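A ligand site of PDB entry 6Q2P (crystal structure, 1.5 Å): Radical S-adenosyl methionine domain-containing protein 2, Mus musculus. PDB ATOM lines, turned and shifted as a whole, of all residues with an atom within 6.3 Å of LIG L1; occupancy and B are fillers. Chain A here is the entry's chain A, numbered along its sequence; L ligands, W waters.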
ATOM      1  N   ARG A  38      19.514  -1.646  22.554  1.00  0.00           N
ATOM      2  CA  ARG A  38      19.572  -2.941  21.886  1.00  0.00           C
ATOM      3  C   ARG A  38      18.822  -4.032  22.651  1.00  0.00           C
ATOM      4  O   ARG A  38      18.789  -5.189  22.196  1.00  0.00           O
ATOM      5  CB  ARG A  38      21.026  -3.359  21.622  1.00  0.00           C
ATOM      6  CG  ARG A  38      21.659  -2.576  20.458  1.00  0.00           C
ATOM      7  CD  ARG A  38      23.105  -3.015  20.281  1.00  0.00           C
ATOM      8  NE  ARG A  38      23.748  -2.499  19.072  1.00  0.00           N
ATOM      9  CZ  ARG A  38      23.765  -3.133  17.902  1.00  0.00           C
ATOM     10  NH1 ARG A  38      23.150  -4.309  17.754  1.00  0.00           N
ATOM     11  NH2 ARG A  38      24.409  -2.610  16.872  1.00  0.00           N
ATOM     12  N   GLN A  39      18.207  -3.703  23.781  1.00  0.00           N
ATOM     13  CA  GLN A  39      17.400  -4.670  24.498  1.00  0.00           C
ATOM     14  C   GLN A  39      16.145  -4.978  23.696  1.00  0.00           C
ATOM     15  O   GLN A  39      15.559  -4.085  23.082  1.00  0.00           O
ATOM     16  CB  GLN A  39      16.997  -4.109  25.850  1.00  0.00           C
ATOM     17  CG  GLN A  39      16.414  -5.173  26.785  1.00  0.00           C
ATOM     18  CD  GLN A  39      15.736  -4.601  28.008  1.00  0.00           C
ATOM     19  OE1 GLN A  39      15.767  -3.400  28.243  1.00  0.00           O
ATOM     20  NE2 GLN A  39      15.081  -5.469  28.764  1.00  0.00           N
ATOM     21  N   CYS A  40      15.708  -6.228  23.712  1.00  0.00           N
ATOM     22  CA  CYS A  40      14.408  -6.577  23.151  1.00  0.00           C
ATOM     23  C   CYS A  40      13.749  -7.662  23.990  1.00  0.00           C
ATOM     24  O   CYS A  40      14.408  -8.422  24.706  1.00  0.00           O
ATOM     25  CB  CYS A  40      14.495  -7.056  21.702  1.00  0.00           C
ATOM     26  SG  CYS A  40      12.862  -7.046  20.928  1.00  0.00           S
ATOM     27  N   ASN A  41      12.420  -7.716  23.895  1.00  0.00           N
ATOM     28  CA  ASN A  41      11.624  -8.743  24.561  1.00  0.00           C
ATOM     29  C   ASN A  41      11.130  -9.837  23.611  1.00  0.00           C
ATOM     30  O   ASN A  41      10.523 -10.807  24.081  1.00  0.00           O
ATOM     31  CB  ASN A  41      10.445  -8.109  25.327  1.00  0.00           C
ATOM     32  CG  ASN A  41       9.468  -7.366  24.416  1.00  0.00           C
ATOM     33  OD1 ASN A  41       9.836  -6.877  23.356  1.00  0.00           O
ATOM     34  ND2 ASN A  41       8.220  -7.290  24.848  1.00  0.00           N
ATOM     35  N   TYR A  42      11.407  -9.716  22.314  1.00  0.00           N
ATOM     36  CA  TYR A  42      11.051 -10.717  21.308  1.00  0.00           C
ATOM     37  C   TYR A  42      12.321 -11.450  20.868  1.00  0.00           C
ATOM     38  O   TYR A  42      13.430 -11.124  21.281  1.00  0.00           O
ATOM     39  CB  TYR A  42      10.384 -10.070  20.095  1.00  0.00           C
ATOM     40  CG  TYR A  42       8.896  -9.819  20.235  1.00  0.00           C
ATOM     41  CD1 TYR A  42       8.241  -9.968  21.457  1.00  0.00           C
ATOM     42  CD2 TYR A  42       8.147  -9.451  19.133  1.00  0.00           C
ATOM     43  CE1 TYR A  42       6.870  -9.742  21.554  1.00  0.00           C
ATOM     44  CE2 TYR A  42       6.795  -9.232  19.221  1.00  0.00           C
ATOM     45  CZ  TYR A  42       6.164  -9.366  20.426  1.00  0.00           C
ATOM     46  OH  TYR A  42       4.809  -9.155  20.503  1.00  0.00           O
ATOM     47  N   LYS A  43      12.139 -12.453  19.979  1.00  0.00           N
ATOM     48  CA  LYS A  43      13.225 -13.357  19.618  1.00  0.00           C
ATOM     49  C   LYS A  43      13.289 -13.621  18.129  1.00  0.00           C
ATOM     50  O   LYS A  43      13.679 -14.715  17.706  1.00  0.00           O
ATOM     51  CB  LYS A  43      13.108 -14.688  20.380  1.00  0.00           C
ATOM     52  CG  LYS A  43      13.408 -14.548  21.847  1.00  0.00           C
ATOM     53  CD  LYS A  43      13.432 -15.890  22.550  1.00  0.00           C
ATOM     54  CE  LYS A  43      12.055 -16.397  22.854  1.00  0.00           C
ATOM     55  NZ  LYS A  43      12.138 -17.380  23.992  1.00  0.00           N
ATOM     56  N   CYS A  44      12.933 -12.634  17.301  1.00  0.00           N
ATOM     57  CA  CYS A  44      12.830 -12.856  15.867  1.00  0.00           C
ATOM     58  C   CYS A  44      14.120 -13.460  15.328  1.00  0.00           C
ATOM     59  O   CYS A  44      15.208 -12.933  15.554  1.00  0.00           O
ATOM     60  CB  CYS A  44      12.525 -11.544  15.150  1.00  0.00           C
ATOM     61  SG  CYS A  44      11.123 -10.654  15.844  1.00  0.00           S
ATOM     62  N   GLY A  45      13.998 -14.602  14.636  1.00  0.00           N
ATOM     63  CA  GLY A  45      15.193 -15.358  14.276  1.00  0.00           C
ATOM     64  C   GLY A  45      16.108 -14.668  13.286  1.00  0.00           C
ATOM     65  O   GLY A  45      17.287 -15.029  13.201  1.00  0.00           O
ATOM     66  N   PHE A  46      15.588 -13.706  12.528  1.00  0.00           N
ATOM     67  CA  PHE A  46      16.384 -12.972  11.552  1.00  0.00           C
ATOM     68  C   PHE A  46      16.872 -11.623  12.057  1.00  0.00           C
ATOM     69  O   PHE A  46      17.476 -10.879  11.292  1.00  0.00           O
ATOM     70  CB  PHE A  46      15.571 -12.744  10.256  1.00  0.00           C
ATOM     71  CG  PHE A  46      14.202 -12.151  10.493  1.00  0.00           C
ATOM     72  CD1 PHE A  46      14.058 -10.857  10.986  1.00  0.00           C
ATOM     73  CD2 PHE A  46      13.059 -12.890  10.241  1.00  0.00           C
ATOM     74  CE1 PHE A  46      12.794 -10.321  11.223  1.00  0.00           C
ATOM     75  CE2 PHE A  46      11.794 -12.354  10.478  1.00  0.00           C
ATOM     76  CZ  PHE A  46      11.666 -11.065  10.952  1.00  0.00           C
ATOM     77  N   CYS A  47      16.603 -11.270  13.317  1.00  0.00           N
ATOM     78  CA  CYS A  47      16.835  -9.907  13.807  1.00  0.00           C
ATOM     79  C   CYS A  47      18.209  -9.396  13.406  1.00  0.00           C
ATOM     80  O   CYS A  47      19.230 -10.024  13.697  1.00  0.00           O
ATOM     81  CB  CYS A  47      16.719  -9.900  15.322  1.00  0.00           C
ATOM     82  SG  CYS A  47      16.959  -8.224  16.003  1.00  0.00           S
ATOM     83  N   PHE A  48      18.237  -8.230  12.751  1.00  0.00           N
ATOM     84  CA  PHE A  48      19.493  -7.617  12.333  1.00  0.00           C
ATOM     85  C   PHE A  48      19.971  -6.495  13.252  1.00  0.00           C
ATOM     86  O   PHE A  48      20.921  -5.791  12.912  1.00  0.00           O
ATOM     87  CB  PHE A  48      19.505  -7.209  10.835  1.00  0.00           C
ATOM     88  CG  PHE A  48      18.551  -6.070  10.448  1.00  0.00           C
ATOM     89  CD1 PHE A  48      17.821  -5.346  11.386  1.00  0.00           C
ATOM     90  CD2 PHE A  48      18.419  -5.740   9.112  1.00  0.00           C
ATOM     91  CE1 PHE A  48      16.957  -4.310  10.972  1.00  0.00           C
ATOM     92  CE2 PHE A  48      17.577  -4.713   8.698  1.00  0.00           C
ATOM     93  CZ  PHE A  48      16.839  -4.010   9.634  1.00  0.00           C
ATOM     94  N   HIS A  49      19.355  -6.333  14.431  1.00  0.00           N
ATOM     95  CA  HIS A  49      19.797  -5.300  15.366  1.00  0.00           C
ATOM     96  C   HIS A  49      19.666  -5.865  16.776  1.00  0.00           C
ATOM     97  O   HIS A  49      18.700  -5.572  17.498  1.00  0.00           O
ATOM     98  CB  HIS A  49      19.079  -3.967  15.194  1.00  0.00           C
ATOM     99  CG  HIS A  49      19.867  -2.821  15.740  1.00  0.00           C
ATOM    100  ND1 HIS A  49      20.802  -2.142  15.003  1.00  0.00           N
ATOM    101  CD2 HIS A  49      19.928  -2.298  16.996  1.00  0.00           C
ATOM    102  CE1 HIS A  49      21.390  -1.234  15.762  1.00  0.00           C
ATOM    103  NE2 HIS A  49      20.883  -1.312  16.974  1.00  0.00           N
ATOM    104  N   THR A  50      20.662  -6.666  17.136  1.00  0.00           N
ATOM    105  CA  THR A  50      20.586  -7.616  18.236  1.00  0.00           C
ATOM    106  C   THR A  50      21.084  -7.039  19.559  1.00  0.00           C
ATOM    107  O   THR A  50      21.641  -5.950  19.634  1.00  0.00           O
ATOM    108  CB  THR A  50      21.368  -8.885  17.878  1.00  0.00           C
ATOM    109  OG1 THR A  50      22.754  -8.565  17.703  1.00  0.00           O
ATOM    110  CG2 THR A  50      20.817  -9.526  16.593  1.00  0.00           C
ATOM    111  N   GLY A  81      15.436   0.226  17.640  1.00  0.00           N
ATOM    112  CA  GLY A  81      16.205  -0.565  18.580  1.00  0.00           C
ATOM    113  C   GLY A  81      16.574  -1.908  17.952  1.00  0.00           C
ATOM    114  O   GLY A  81      16.844  -1.947  16.753  1.00  0.00           O
ATOM    115  N   GLY A  82      16.553  -3.017  18.706  1.00  0.00           N
ATOM    116  CA  GLY A  82      15.958  -3.086  20.032  1.00  0.00           C
ATOM    117  C   GLY A  82      14.464  -2.760  20.037  1.00  0.00           C
ATOM    118  O   GLY A  82      13.897  -2.369  19.000  1.00  0.00           O
ATOM    119  N   GLU A  83      13.824  -2.891  21.191  1.00  0.00           N
ATOM    120  CA  GLU A  83      12.429  -2.498  21.315  1.00  0.00           C
ATOM    121  C   GLU A  83      12.369  -1.177  22.045  1.00  0.00           C
ATOM    122  O   GLU A  83      12.632  -1.140  23.260  1.00  0.00           O
ATOM    123  CB  GLU A  83      11.602  -3.559  22.030  1.00  0.00           C
ATOM    124  CG  GLU A  83      10.158  -3.128  22.326  1.00  0.00           C
ATOM    125  CD  GLU A  83       9.485  -2.465  21.130  1.00  0.00           C
ATOM    126  OE1 GLU A  83       9.668  -2.956  19.993  1.00  0.00           O
ATOM    127  OE2 GLU A  83       8.804  -1.429  21.326  1.00  0.00           O
ATOM    128  N   SER A 113       8.209  -0.150  16.250  1.00  0.00           N
ATOM    129  CA  SER A 113       8.078  -0.935  17.465  1.00  0.00           C
ATOM    130  C   SER A 113       7.454  -2.291  17.168  1.00  0.00           C
ATOM    131  O   SER A 113       6.672  -2.429  16.227  1.00  0.00           O
ATOM    132  CB  SER A 113       7.190  -0.169  18.454  1.00  0.00           C
ATOM    133  OG  SER A 113       6.843  -0.952  19.580  1.00  0.00           O
ATOM    134  N   ASN A 114       7.772  -3.283  18.011  1.00  0.00           N
ATOM    135  CA  ASN A 114       7.067  -4.563  17.930  1.00  0.00           C
ATOM    136  C   ASN A 114       5.651  -4.504  18.481  1.00  0.00           C
ATOM    137  O   ASN A 114       4.890  -5.464  18.310  1.00  0.00           O
ATOM    138  CB  ASN A 114       7.886  -5.737  18.517  1.00  0.00           C
ATOM    139  CG  ASN A 114       8.059  -5.681  20.049  1.00  0.00           C
ATOM    140  OD1 ASN A 114       7.237  -5.102  20.769  1.00  0.00           O
ATOM    141  ND2 ASN A 114       9.120  -6.304  20.535  1.00  0.00           N
ATOM    142  N   SER A 136       5.722  -3.489  13.626  1.00  0.00           N
ATOM    143  CA  SER A 136       6.213  -4.584  12.809  1.00  0.00           C
ATOM    144  C   SER A 136       5.262  -5.758  12.885  1.00  0.00           C
ATOM    145  O   SER A 136       4.889  -6.204  13.979  1.00  0.00           O
ATOM    146  CB  SER A 136       7.631  -4.991  13.235  1.00  0.00           C
ATOM    147  OG  SER A 136       8.518  -3.927  12.972  1.00  0.00           O
ATOM    148  N   GLY A 149       9.480 -16.082  15.769  1.00  0.00           N
ATOM    149  CA  GLY A 149       9.879 -15.618  17.073  1.00  0.00           C
ATOM    150  C   GLY A 149       9.274 -14.285  17.496  1.00  0.00           C
ATOM    151  O   GLY A 149       9.830 -13.640  18.393  1.00  0.00           O
ATOM    152  N   ARG A 150       8.180 -13.858  16.878  1.00  0.00           N
ATOM    153  CA  ARG A 150       7.482 -12.619  17.250  1.00  0.00           C
ATOM    154  C   ARG A 150       6.569 -12.901  18.423  1.00  0.00           C
ATOM    155  O   ARG A 150       5.387 -13.218  18.251  1.00  0.00           O
ATOM    156  CB  ARG A 150       6.648 -12.124  16.080  1.00  0.00           C
ATOM    157  CG  ARG A 150       7.418 -11.536  14.980  1.00  0.00           C
ATOM    158  CD  ARG A 150       7.680 -10.050  15.189  1.00  0.00           C
ATOM    159  NE  ARG A 150       8.372  -9.552  14.022  1.00  0.00           N
ATOM    160  CZ  ARG A 150       9.070  -8.428  13.938  1.00  0.00           C
ATOM    161  NH1 ARG A 150       9.191  -7.599  14.975  1.00  0.00           N
ATOM    162  NH2 ARG A 150       9.670  -8.135  12.793  1.00  0.00           N
ATOM    163  N   ARG A 221      22.210 -13.993  16.214  1.00  0.00           N
ATOM    164  CA  ARG A 221      21.181 -14.621  15.412  1.00  0.00           C
ATOM    165  C   ARG A 221      21.816 -15.233  14.175  1.00  0.00           C
ATOM    166  O   ARG A 221      22.976 -14.954  13.839  1.00  0.00           O
ATOM    167  CB  ARG A 221      20.091 -13.619  15.015  1.00  0.00           C
ATOM    168  CG  ARG A 221      19.378 -13.012  16.216  1.00  0.00           C
ATOM    169  CD  ARG A 221      18.507 -14.039  16.911  1.00  0.00           C
ATOM    170  NE  ARG A 221      17.812 -13.486  18.082  1.00  0.00           N
ATOM    171  CZ  ARG A 221      18.059 -13.824  19.348  1.00  0.00           C
ATOM    172  NH1 ARG A 221      19.000 -14.724  19.642  1.00  0.00           N
ATOM    173  NH2 ARG A 221      17.352 -13.252  20.318  1.00  0.00           N
HETATM  174 FE1  LIG L   1      13.242  -7.413  18.715  1.00  0.00          FE
HETATM  175 FE2  LIG L   1      12.239  -8.735  16.571  1.00  0.00          FE
HETATM  176 FE3  LIG L   1      14.739  -7.680  16.539  1.00  0.00          FE
HETATM  177 FE4  LIG L   1      12.446  -5.954  16.586  1.00  0.00          FE
HETATM  178  S1  LIG L   1      13.146  -7.462  14.904  1.00  0.00           S
HETATM  179  S2  LIG L   1      14.568  -5.858  17.761  1.00  0.00           S
HETATM  180  S3  LIG L   1      11.078  -7.352  17.891  1.00  0.00           S
HETATM  181  S4  LIG L   1      14.002  -9.371  17.930  1.00  0.00           S
HETATM  182  N1  LG2 L   2      12.003  -3.975  17.712  1.00  0.00           N
HETATM  183  C1  LG2 L   2      11.349  -3.057  16.778  1.00  0.00           C
HETATM  184  C2  LG2 L   2      12.332  -2.070  16.138  1.00  0.00           C
HETATM  185  C3  LG2 L   2      13.722  -2.651  15.817  1.00  0.00           C
HETATM  186  S1  LG2 L   2      13.801  -3.590  14.265  1.00  0.00           S
HETATM  187  C4  LG2 L   2      10.604  -3.821  15.708  1.00  0.00           C
HETATM  188  O1  LG2 L   2      10.797  -5.003  15.475  1.00  0.00           O
HETATM  189  O2  LG2 L   2       9.680  -3.182  15.016  1.00  0.00           O
HETATM  190  C5  LG2 L   2      13.438  -2.306  13.034  1.00  0.00           C
HETATM  191  C6  LG2 L   2      12.786  -2.882  11.761  1.00  0.00           C
HETATM  192  O3  LG2 L   2      13.727  -3.744  11.081  1.00  0.00           O
HETATM  193  C7  LG2 L   2      11.525  -3.709  12.087  1.00  0.00           C
HETATM  194  O4  LG2 L   2      10.479  -3.374  11.186  1.00  0.00           O
HETATM  195  C8  LG2 L   2      12.026  -5.165  11.887  1.00  0.00           C
HETATM  196  O5  LG2 L   2      10.976  -6.084  11.588  1.00  0.00           O
HETATM  197  C9  LG2 L   2      13.025  -4.952  10.718  1.00  0.00           C
HETATM  198  N2  LG2 L   2      13.993  -6.036  10.638  1.00  0.00           N
HETATM  199  C10 LG2 L   2      14.567  -6.743  11.664  1.00  0.00           C
HETATM  200  N3  LG2 L   2      15.403  -7.629  11.187  1.00  0.00           N
HETATM  201  C11 LG2 L   2      15.417  -7.513   9.819  1.00  0.00           C
HETATM  202  C12 LG2 L   2      16.088  -8.181   8.774  1.00  0.00           C
HETATM  203  N4  LG2 L   2      16.971  -9.191   9.043  1.00  0.00           N
HETATM  204  N5  LG2 L   2      15.848  -7.784   7.519  1.00  0.00           N
HETATM  205  C13 LG2 L   2      14.989  -6.803   7.245  1.00  0.00           C
HETATM  206  N6  LG2 L   2      14.327  -6.151   8.193  1.00  0.00           N
HETATM  207  C14 LG2 L   2      14.524  -6.493   9.468  1.00  0.00           C
HETATM  208  O   HOH W   1      15.994 -11.803  17.972  1.00  0.00           O
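An oxygen (O1) of LG2 L2 binds an iron atom (FE4) of LIG L1, 2.2 Å away.
Water W1 lies within hydrogen-bond range of the guanidinium group (NE) of Arg 221 (2.5 Å), the backbone carbonyl oxygen (O) of Cys 44 (2.8 Å) and a sulfur (S4) of LIG L1 (3.1 Å).
A nitrogen (N3) of LG2 L2 is in hydrogen-bond range of the backbone NH (N) of Phe 48. OG of Ser 136 lies within hydrogen-bond range of O2 of LG2 L2, 2.5 Å away. The side-chain sulfur (SG) of Cys 44 is bound to an iron atom (FE2) of LIG L1, 2.3 Å away. N of Gly 82 lies close to S2 of LIG L1 (3.6 Å). O of Gly 82 lies close to N1 of LG2 L2. A sulfur (S3) of LIG L1 sits close to the side-chain amide nitrogen of Asn 114, at 3.5 Å. The backbone NH (N) of Cys 44 lies close to a sulfur (S4) of LIG L1, at 3.5 Å. SG of Cys 40 binds FE1 of LIG L1 (2.3 Å). The side-chain sulfur (SG) of Cys 47 binds an iron atom (FE3) of LIG L1, 2.3 Å away. The side-chain carboxylate (OE1) of Glu 83 sits close to a nitrogen (N1) of LG2 L2 (3.4 Å). The backbone carbonyl oxygen (O) of Phe 46 sits at hydrogen-bond distance from a nitrogen (N4) of LG2 L2 (2.9 Å). An oxygen (O5) of LG2 L2 lies within hydrogen-bond range of the guanidinium group (NH2) of Arg 150, 2.7 Å away. The guanidinium group of Arg 150 lies close to a sulfur (S3) of LIG L1, 3.5 Å away.
N of His 49 sits close to SG of Cys 47 (3.4 Å). The backbone carbonyl oxygen of Gly 149 sits at hydrogen-bond distance from the backbone NH of Cys 44, 3.4 Å away. The side-chain sulfur (SG) of Cys 44 lies close to the guanidinium group (NE) of Arg 150, at 3.5 Å. The backbone NH of Asn 114 is in hydrogen-bond range of the side-chain carboxylate of Glu 83. The side-chain amide oxygen (OD1) of Asn 41 is in hydrogen-bond range of the side-chain amide nitrogen (ND2) of Asn 114 (3.0 Å). The backbone NH of Tyr 42 lies close to the side-chain sulfur of Cys 40, at 3.3 Å.
Tyr 42 touches LIG L1.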
